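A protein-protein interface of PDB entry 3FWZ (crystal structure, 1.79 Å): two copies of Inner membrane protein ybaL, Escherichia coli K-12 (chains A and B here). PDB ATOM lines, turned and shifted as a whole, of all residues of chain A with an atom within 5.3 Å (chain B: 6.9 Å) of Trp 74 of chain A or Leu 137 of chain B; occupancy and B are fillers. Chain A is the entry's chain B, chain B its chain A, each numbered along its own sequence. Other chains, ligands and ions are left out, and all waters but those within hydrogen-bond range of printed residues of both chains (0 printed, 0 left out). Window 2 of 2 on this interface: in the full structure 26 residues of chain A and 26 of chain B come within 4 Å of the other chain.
N of Trp 74 of chain A lies within hydrogen-bond range of O of His 9 of chain A (3.3 Å).
The backbone carbonyl oxygen (O) of Leu 11 of chain A is in hydrogen-bond range of the backbone NH (N) of Ile 76 of chain A (2.8 Å).
The backbone carbonyl oxygen of Trp 74 of chain A is in hydrogen-bond range of the backbone NH of Leu 11 of chain A, 3.0 Å away.
The backbone carbonyl oxygen of Leu 75 of chain A lies within hydrogen-bond range of the backbone NH of Ile 102 of chain A, 3.0 Å away.
Leu 22 of chain A touches Met 133 of chain B (CD2 to SD, 3.7 Å).
N of Leu 134 of chain B touches CD1 of Leu 22 of chain A, 3.97 Å away.
CD1 of Leu 22 of chain A touches CD1 of Leu 137 of chain B, at 3.9 Å.
CD1 of Trp 74 of chain A touches CD2 of Leu 137 of chain B, 3.4 Å away.
Ile 76 of chain A touches Leu 137 of chain B (CD1 to CD1, 3.9 Å).
CD1 of Ile 102 of chain A touches CD2 of Leu 137 of chain B, 3.4 Å away.
Trp 74 of chain A touches one residue of chain B.
Printed residues of chain A within 4 Å of Leu 137 of chain B: Leu 22, Trp 74, Ile 76 and Ile 102.
Printed residues of chain A within 4 Å of Met 133 of chain B: Leu 22.
Of the printed residues of chain B, Leu 22 of chain A touches Met 133, Leu 134 and Leu 137.
Of the printed residues of chain B, Ile 76 of chain A touches Leu 137.
Ala 10 of chain A touches none of the printed residues of chain B.
His 9 of chain A touches none of the printed residues of chain B.
The nearest residue of chain B that does not touch Trp 74 of chain A is Leu 136 of chain B (6.4 Å).
The nearest printed residue of chain B that does not touch Ile 76 of chain A is Met 133 of chain B (4.1 Å).
Hydrophobic or aromatic side chains of chain A that line the printed part of chain B: Leu 22, Trp 74, Ile 76 and Ile 102.
Along chain A the printed residues that touch a printed residue of chain B span positions 22 to 102.
Printed residues of chain B that touch a printed residue of chain A: Met 133, Leu 134 and Leu 137.
Hydrophobic or aromatic side chains of chain B that line the printed part of chain A: Met 133 and Leu 137.
Among the printed residues, 6 pairs touch across the chains.
No position is printed for both chains.
Of the 6 pairs that touch across the chains among the printed residues, none has its exchanged pair printed and touching as well.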
ATOM      1  N   ASN A   8     -10.246 -22.596  -3.285  1.00  0.00           N
ATOM      2  CA  ASN A   8      -8.913 -22.944  -3.828  1.00  0.00           C
ATOM      3  C   ASN A   8      -7.786 -22.006  -3.437  1.00  0.00           C
ATOM      4  O   ASN A   8      -6.791 -21.871  -4.147  1.00  0.00           O
ATOM      5  CB  ASN A   8      -8.969 -23.130  -5.346  1.00  0.00           C
ATOM      6  CG  ASN A   8     -10.097 -24.012  -5.761  1.00  0.00           C
ATOM      7  OD1 ASN A   8     -10.331 -25.067  -5.165  1.00  0.00           O
ATOM      8  ND2 ASN A   8     -10.832 -23.584  -6.768  1.00  0.00           N
ATOM      9  N   HIS A   9      -7.937 -21.359  -2.282  1.00  0.00           N
ATOM     10  CA  HIS A   9      -6.997 -20.347  -1.841  1.00  0.00           C
ATOM     11  C   HIS A   9      -5.949 -20.911  -0.879  1.00  0.00           C
ATOM     12  O   HIS A   9      -6.119 -22.020  -0.330  1.00  0.00           O
ATOM     13  CB  HIS A   9      -7.759 -19.237  -1.110  1.00  0.00           C
ATOM     14  CG  HIS A   9      -8.707 -19.740  -0.062  1.00  0.00           C
ATOM     15  ND1 HIS A   9      -9.737 -20.608  -0.347  1.00  0.00           N
ATOM     16  CD2 HIS A   9      -8.787 -19.486   1.263  1.00  0.00           C
ATOM     17  CE1 HIS A   9     -10.407 -20.875   0.757  1.00  0.00           C
ATOM     18  NE2 HIS A   9      -9.853 -20.204   1.750  1.00  0.00           N
ATOM     19  N   ALA A  10      -4.895 -20.120  -0.664  1.00  0.00           N
ATOM     20  CA  ALA A  10      -3.969 -20.332   0.428  1.00  0.00           C
ATOM     21  C   ALA A  10      -4.605 -19.728   1.685  1.00  0.00           C
ATOM     22  O   ALA A  10      -5.023 -18.575   1.690  1.00  0.00           O
ATOM     23  CB  ALA A  10      -2.623 -19.708   0.129  1.00  0.00           C
ATOM     24  N   LEU A  11      -4.721 -20.551   2.716  1.00  0.00           N
ATOM     25  CA  LEU A  11      -5.287 -20.165   3.986  1.00  0.00           C
ATOM     26  C   LEU A  11      -4.096 -20.122   4.924  1.00  0.00           C
ATOM     27  O   LEU A  11      -3.532 -21.146   5.299  1.00  0.00           O
ATOM     28  CB  LEU A  11      -6.349 -21.195   4.408  1.00  0.00           C
ATOM     29  CG  LEU A  11      -7.046 -20.907   5.756  1.00  0.00           C
ATOM     30  CD1 LEU A  11      -7.341 -19.422   5.992  1.00  0.00           C
ATOM     31  CD2 LEU A  11      -8.332 -21.708   5.858  1.00  0.00           C
ATOM     32  N   LEU A  22       5.836 -14.604   4.086  1.00  0.00           N
ATOM     33  CA  LEU A  22       5.212 -15.524   3.161  1.00  0.00           C
ATOM     34  C   LEU A  22       4.029 -14.881   2.426  1.00  0.00           C
ATOM     35  O   LEU A  22       3.902 -14.998   1.200  1.00  0.00           O
ATOM     36  CB  LEU A  22       4.752 -16.744   3.942  1.00  0.00           C
ATOM     37  CG  LEU A  22       4.332 -18.031   3.263  1.00  0.00           C
ATOM     38  CD1 LEU A  22       5.281 -18.402   2.146  1.00  0.00           C
ATOM     39  CD2 LEU A  22       4.341 -19.079   4.307  1.00  0.00           C
ATOM     40  N   LEU A  26       3.209 -14.514  -1.622  1.00  0.00           N
ATOM     41  CA  LEU A  26       1.976 -15.085  -2.178  1.00  0.00           C
ATOM     42  C   LEU A  26       1.141 -14.019  -2.881  1.00  0.00           C
ATOM     43  O   LEU A  26       0.708 -14.237  -4.009  1.00  0.00           O
ATOM     44  CB  LEU A  26       1.162 -15.833  -1.103  1.00  0.00           C
ATOM     45  CG  LEU A  26       1.853 -17.092  -0.551  1.00  0.00           C
ATOM     46  CD1 LEU A  26       1.170 -17.615   0.711  1.00  0.00           C
ATOM     47  CD2 LEU A  26       1.933 -18.208  -1.588  1.00  0.00           C
ATOM     48  N   ILE A  31      -1.515 -15.448  -5.794  1.00  0.00           N
ATOM     49  CA  ILE A  31      -2.117 -16.642  -5.193  1.00  0.00           C
ATOM     50  C   ILE A  31      -3.272 -16.146  -4.339  1.00  0.00           C
ATOM     51  O   ILE A  31      -3.058 -15.264  -3.503  1.00  0.00           O
ATOM     52  CB  ILE A  31      -1.080 -17.429  -4.318  1.00  0.00           C
ATOM     53  CG1 ILE A  31       0.146 -17.827  -5.168  1.00  0.00           C
ATOM     54  CG2 ILE A  31      -1.723 -18.641  -3.652  1.00  0.00           C
ATOM     55  CD1 ILE A  31      -0.199 -18.594  -6.475  1.00  0.00           C
ATOM     56  N   ALA A  72     -10.371 -24.627   0.856  1.00  0.00           N
ATOM     57  CA  ALA A  72      -9.051 -24.073   0.594  1.00  0.00           C
ATOM     58  C   ALA A  72      -8.127 -25.099  -0.069  1.00  0.00           C
ATOM     59  O   ALA A  72      -8.298 -26.313   0.114  1.00  0.00           O
ATOM     60  CB  ALA A  72      -8.414 -23.538   1.916  1.00  0.00           C
ATOM     61  N   LYS A  73      -7.135 -24.612  -0.804  1.00  0.00           N
ATOM     62  CA  LYS A  73      -6.134 -25.483  -1.410  1.00  0.00           C
ATOM     63  C   LYS A  73      -4.973 -25.817  -0.490  1.00  0.00           C
ATOM     64  O   LYS A  73      -4.550 -26.980  -0.421  1.00  0.00           O
ATOM     65  CB  LYS A  73      -5.565 -24.892  -2.681  1.00  0.00           C
ATOM     66  CG  LYS A  73      -5.052 -25.986  -3.560  1.00  0.00           C
ATOM     67  CD  LYS A  73      -3.807 -25.585  -4.255  1.00  0.00           C
ATOM     68  CE  LYS A  73      -4.106 -24.928  -5.567  1.00  0.00           C
ATOM     69  NZ  LYS A  73      -3.116 -25.432  -6.544  1.00  0.00           N
ATOM     70  N   TRP A  74      -4.425 -24.794   0.182  1.00  0.00           N
ATOM     71  CA  TRP A  74      -3.338 -25.030   1.136  1.00  0.00           C
ATOM     72  C   TRP A  74      -3.757 -24.475   2.485  1.00  0.00           C
ATOM     73  O   TRP A  74      -4.469 -23.490   2.571  1.00  0.00           O
ATOM     74  CB  TRP A  74      -2.041 -24.285   0.775  1.00  0.00           C
ATOM     75  CG  TRP A  74      -1.427 -24.529  -0.582  1.00  0.00           C
ATOM     76  CD1 TRP A  74      -0.452 -25.425  -0.893  1.00  0.00           C
ATOM     77  CD2 TRP A  74      -1.686 -23.786  -1.765  1.00  0.00           C
ATOM     78  NE1 TRP A  74      -0.110 -25.313  -2.216  1.00  0.00           N
ATOM     79  CE2 TRP A  74      -0.849 -24.308  -2.776  1.00  0.00           C
ATOM     80  CE3 TRP A  74      -2.559 -22.733  -2.074  1.00  0.00           C
ATOM     81  CZ2 TRP A  74      -0.855 -23.813  -4.082  1.00  0.00           C
ATOM     82  CZ3 TRP A  74      -2.562 -22.228  -3.367  1.00  0.00           C
ATOM     83  CH2 TRP A  74      -1.713 -22.781  -4.360  1.00  0.00           C
ATOM     84  N   LEU A  75      -3.274 -25.113   3.529  1.00  0.00           N
ATOM     85  CA  LEU A  75      -3.339 -24.537   4.850  1.00  0.00           C
ATOM     86  C   LEU A  75      -1.903 -24.353   5.260  1.00  0.00           C
ATOM     87  O   LEU A  75      -1.135 -25.317   5.257  1.00  0.00           O
ATOM     88  CB  LEU A  75      -4.044 -25.500   5.828  1.00  0.00           C
ATOM     89  CG  LEU A  75      -4.069 -25.058   7.295  1.00  0.00           C
ATOM     90  CD1 LEU A  75      -4.852 -23.735   7.482  1.00  0.00           C
ATOM     91  CD2 LEU A  75      -4.659 -26.160   8.198  1.00  0.00           C
ATOM     92  N   ILE A  76      -1.554 -23.135   5.643  1.00  0.00           N
ATOM     93  CA  ILE A  76      -0.163 -22.812   5.990  1.00  0.00           C
ATOM     94  C   ILE A  76      -0.156 -22.275   7.410  1.00  0.00           C
ATOM     95  O   ILE A  76      -0.693 -21.201   7.654  1.00  0.00           O
ATOM     96  CB  ILE A  76       0.441 -21.758   5.032  1.00  0.00           C
ATOM     97  CG1 ILE A  76       0.314 -22.220   3.575  1.00  0.00           C
ATOM     98  CG2 ILE A  76       1.915 -21.410   5.444  1.00  0.00           C
ATOM     99  CD1 ILE A  76       0.247 -21.054   2.557  1.00  0.00           C
ATOM    100  N   ILE A  99      -6.542 -31.242   1.562  1.00  0.00           N
ATOM    101  CA  ILE A  99      -5.814 -29.964   1.657  1.00  0.00           C
ATOM    102  C   ILE A  99      -4.298 -30.233   1.870  1.00  0.00           C
ATOM    103  O   ILE A  99      -3.946 -31.175   2.584  1.00  0.00           O
ATOM    104  CB  ILE A  99      -6.444 -29.080   2.766  1.00  0.00           C
ATOM    105  CG1 ILE A  99      -5.980 -27.601   2.666  1.00  0.00           C
ATOM    106  CG2 ILE A  99      -6.236 -29.679   4.162  1.00  0.00           C
ATOM    107  CD1 ILE A  99      -6.793 -26.677   3.575  1.00  0.00           C
ATOM    108  N   GLU A 100      -3.421 -29.458   1.225  1.00  0.00           N
ATOM    109  CA  GLU A 100      -1.980 -29.547   1.477  1.00  0.00           C
ATOM    110  C   GLU A 100      -1.679 -28.694   2.711  1.00  0.00           C
ATOM    111  O   GLU A 100      -1.979 -27.496   2.749  1.00  0.00           O
ATOM    112  CB  GLU A 100      -1.162 -29.038   0.293  1.00  0.00           C
ATOM    113  CG  GLU A 100       0.391 -29.038   0.496  1.00  0.00           C
ATOM    114  CD  GLU A 100       1.088 -30.405   0.244  1.00  0.00           C
ATOM    115  OE1 GLU A 100       0.410 -31.402  -0.045  1.00  0.00           O
ATOM    116  OE2 GLU A 100       2.340 -30.483   0.337  1.00  0.00           O
ATOM    117  N   ILE A 102       1.103 -27.268   5.485  1.00  0.00           N
ATOM    118  CA  ILE A 102       2.489 -26.967   5.812  1.00  0.00           C
ATOM    119  C   ILE A 102       2.442 -26.261   7.165  1.00  0.00           C
ATOM    120  O   ILE A 102       1.500 -25.512   7.450  1.00  0.00           O
ATOM    121  CB  ILE A 102       3.124 -26.020   4.779  1.00  0.00           C
ATOM    122  CG1 ILE A 102       3.055 -26.614   3.377  1.00  0.00           C
ATOM    123  CG2 ILE A 102       4.567 -25.689   5.149  1.00  0.00           C
ATOM    124  CD1 ILE A 102       3.238 -25.595   2.318  1.00  0.00           C
ATOM    125  N   ALA B 130      10.233 -18.764   6.434  1.00  0.00           N
ATOM    126  CA  ALA B 130       9.395 -18.219   5.348  1.00  0.00           C
ATOM    127  C   ALA B 130       9.978 -18.609   3.993  1.00  0.00           C
ATOM    128  O   ALA B 130       9.253 -19.057   3.079  1.00  0.00           O
ATOM    129  CB  ALA B 130       9.281 -16.685   5.489  1.00  0.00           C
ATOM    130  N   THR B 132      11.909 -21.126   3.224  1.00  0.00           N
ATOM    131  CA  THR B 132      11.813 -22.571   2.956  1.00  0.00           C
ATOM    132  C   THR B 132      10.366 -22.937   2.638  1.00  0.00           C
ATOM    133  O   THR B 132      10.111 -23.789   1.769  1.00  0.00           O
ATOM    134  CB  THR B 132      12.369 -23.379   4.176  1.00  0.00           C
ATOM    135  OG1 THR B 132      13.754 -23.080   4.308  1.00  0.00           O
ATOM    136  CG2 THR B 132      12.226 -24.900   3.990  1.00  0.00           C
ATOM    137  N   MET B 133       9.425 -22.342   3.360  1.00  0.00           N
ATOM    138  CA  MET B 133       8.001 -22.595   3.058  1.00  0.00           C
ATOM    139  C   MET B 133       7.626 -22.165   1.639  1.00  0.00           C
ATOM    140  O   MET B 133       6.885 -22.873   0.953  1.00  0.00           O
ATOM    141  CB  MET B 133       7.055 -21.954   4.052  1.00  0.00           C
ATOM    142  CG  MET B 133       7.090 -22.580   5.419  1.00  0.00           C
ATOM    143  SD  MET B 133       5.803 -21.670   6.568  1.00  0.00           S
ATOM    144  CE  MET B 133       5.999 -22.868   8.019  1.00  0.00           C
ATOM    145  N   LEU B 134       8.130 -21.008   1.206  1.00  0.00           N
ATOM    146  CA  LEU B 134       7.867 -20.541  -0.144  1.00  0.00           C
ATOM    147  C   LEU B 134       8.458 -21.522  -1.160  1.00  0.00           C
ATOM    148  O   LEU B 134       7.808 -21.851  -2.169  1.00  0.00           O
ATOM    149  CB  LEU B 134       8.379 -19.111  -0.366  1.00  0.00           C
ATOM    150  CG  LEU B 134       8.193 -18.563  -1.786  1.00  0.00           C
ATOM    151  CD1 LEU B 134       6.734 -18.367  -2.111  1.00  0.00           C
ATOM    152  CD2 LEU B 134       8.957 -17.260  -1.981  1.00  0.00           C
ATOM    153  N   GLU B 135       9.665 -22.021  -0.881  1.00  0.00           N
ATOM    154  CA  GLU B 135      10.265 -23.003  -1.763  1.00  0.00           C
ATOM    155  C   GLU B 135       9.392 -24.234  -1.898  1.00  0.00           C
ATOM    156  O   GLU B 135       9.238 -24.762  -3.010  1.00  0.00           O
ATOM    157  CB  GLU B 135      11.679 -23.360  -1.315  1.00  0.00           C
ATOM    158  CG  GLU B 135      12.643 -22.194  -1.498  1.00  0.00           C
ATOM    159  CD  GLU B 135      13.970 -22.424  -0.804  1.00  0.00           C
ATOM    160  OE1 GLU B 135      14.132 -23.470  -0.149  1.00  0.00           O
ATOM    161  OE2 GLU B 135      14.833 -21.534  -0.881  1.00  0.00           O
ATOM    162  N   LEU B 136       8.838 -24.701  -0.781  1.00  0.00           N
ATOM    163  CA  LEU B 136       7.901 -25.838  -0.826  1.00  0.00           C
ATOM    164  C   LEU B 136       6.648 -25.512  -1.639  1.00  0.00           C
ATOM    165  O   LEU B 136       6.204 -26.337  -2.441  1.00  0.00           O
ATOM    166  CB  LEU B 136       7.491 -26.283   0.586  1.00  0.00           C
ATOM    167  CG  LEU B 136       8.624 -26.863   1.432  1.00  0.00           C
ATOM    168  CD1 LEU B 136       8.144 -27.034   2.878  1.00  0.00           C
ATOM    169  CD2 LEU B 136       9.202 -28.185   0.835  1.00  0.00           C
ATOM    170  N   LEU B 137       6.078 -24.327  -1.412  1.00  0.00           N
ATOM    171  CA  LEU B 137       4.852 -23.914  -2.097  1.00  0.00           C
ATOM    172  C   LEU B 137       5.081 -23.753  -3.599  1.00  0.00           C
ATOM    173  O   LEU B 137       4.174 -24.012  -4.383  1.00  0.00           O
ATOM    174  CB  LEU B 137       4.302 -22.611  -1.491  1.00  0.00           C
ATOM    175  CG  LEU B 137       3.701 -22.818  -0.110  1.00  0.00           C
ATOM    176  CD1 LEU B 137       3.550 -21.483   0.596  1.00  0.00           C
ATOM    177  CD2 LEU B 137       2.320 -23.526  -0.194  1.00  0.00           C
ATOM    178  N   GLU B 138       6.300 -23.369  -3.988  1.00  0.00           N
ATOM    179  CA  GLU B 138       6.636 -23.159  -5.416  1.00  0.00           C
ATOM    180  C   GLU B 138       7.066 -24.414  -6.169  1.00  0.00           C
ATOM    181  O   GLU B 138       7.246 -24.392  -7.397  1.00  0.00           O
ATOM    182  CB  GLU B 138       7.715 -22.094  -5.540  1.00  0.00           C
ATOM    183  CG  GLU B 138       7.209 -20.740  -5.094  1.00  0.00           C
ATOM    184  CD  GLU B 138       8.180 -19.626  -5.369  1.00  0.00           C
ATOM    185  OE1 GLU B 138       9.402 -19.885  -5.446  1.00  0.00           O
ATOM    186  OE2 GLU B 138       7.705 -18.475  -5.479  1.00  0.00           O
ATOM    187  N   THR B 139       7.190 -25.514  -5.440  1.00  0.00           N
ATOM    188  CA  THR B 139       7.560 -26.802  -6.020  1.00  0.00           C
ATOM    189  C   THR B 139       6.339 -27.466  -6.631  1.00  0.00           C
ATOM    190  O   THR B 139       5.297 -27.572  -5.983  1.00  0.00           O
ATOM    191  CB  THR B 139       8.163 -27.721  -4.950  1.00  0.00           C
ATOM    192  OG1 THR B 139       9.309 -27.066  -4.384  1.00  0.00           O
ATOM    193  CG2 THR B 139       8.598 -29.081  -5.573  1.00  0.00           C
ATOM    194  N   PRO B 140       6.461 -27.925  -7.881  1.00  0.00           N
ATOM    195  CA  PRO B 140       5.323 -28.604  -8.515  1.00  0.00           C
ATOM    196  C   PRO B 140       4.890 -29.888  -7.805  1.00  0.00           C
ATOM    197  O   PRO B 140       3.727 -30.302  -7.970  1.00  0.00           O
ATOM    198  CB  PRO B 140       5.825 -28.917  -9.931  1.00  0.00           C
ATOM    199  CG  PRO B 140       7.319 -28.760  -9.898  1.00  0.00           C
ATOM    200  CD  PRO B 140       7.660 -27.862  -8.738  1.00  0.00           C
ATOM    201  OXT PRO B 140       5.648 -30.547  -7.064  1.00  0.00           O
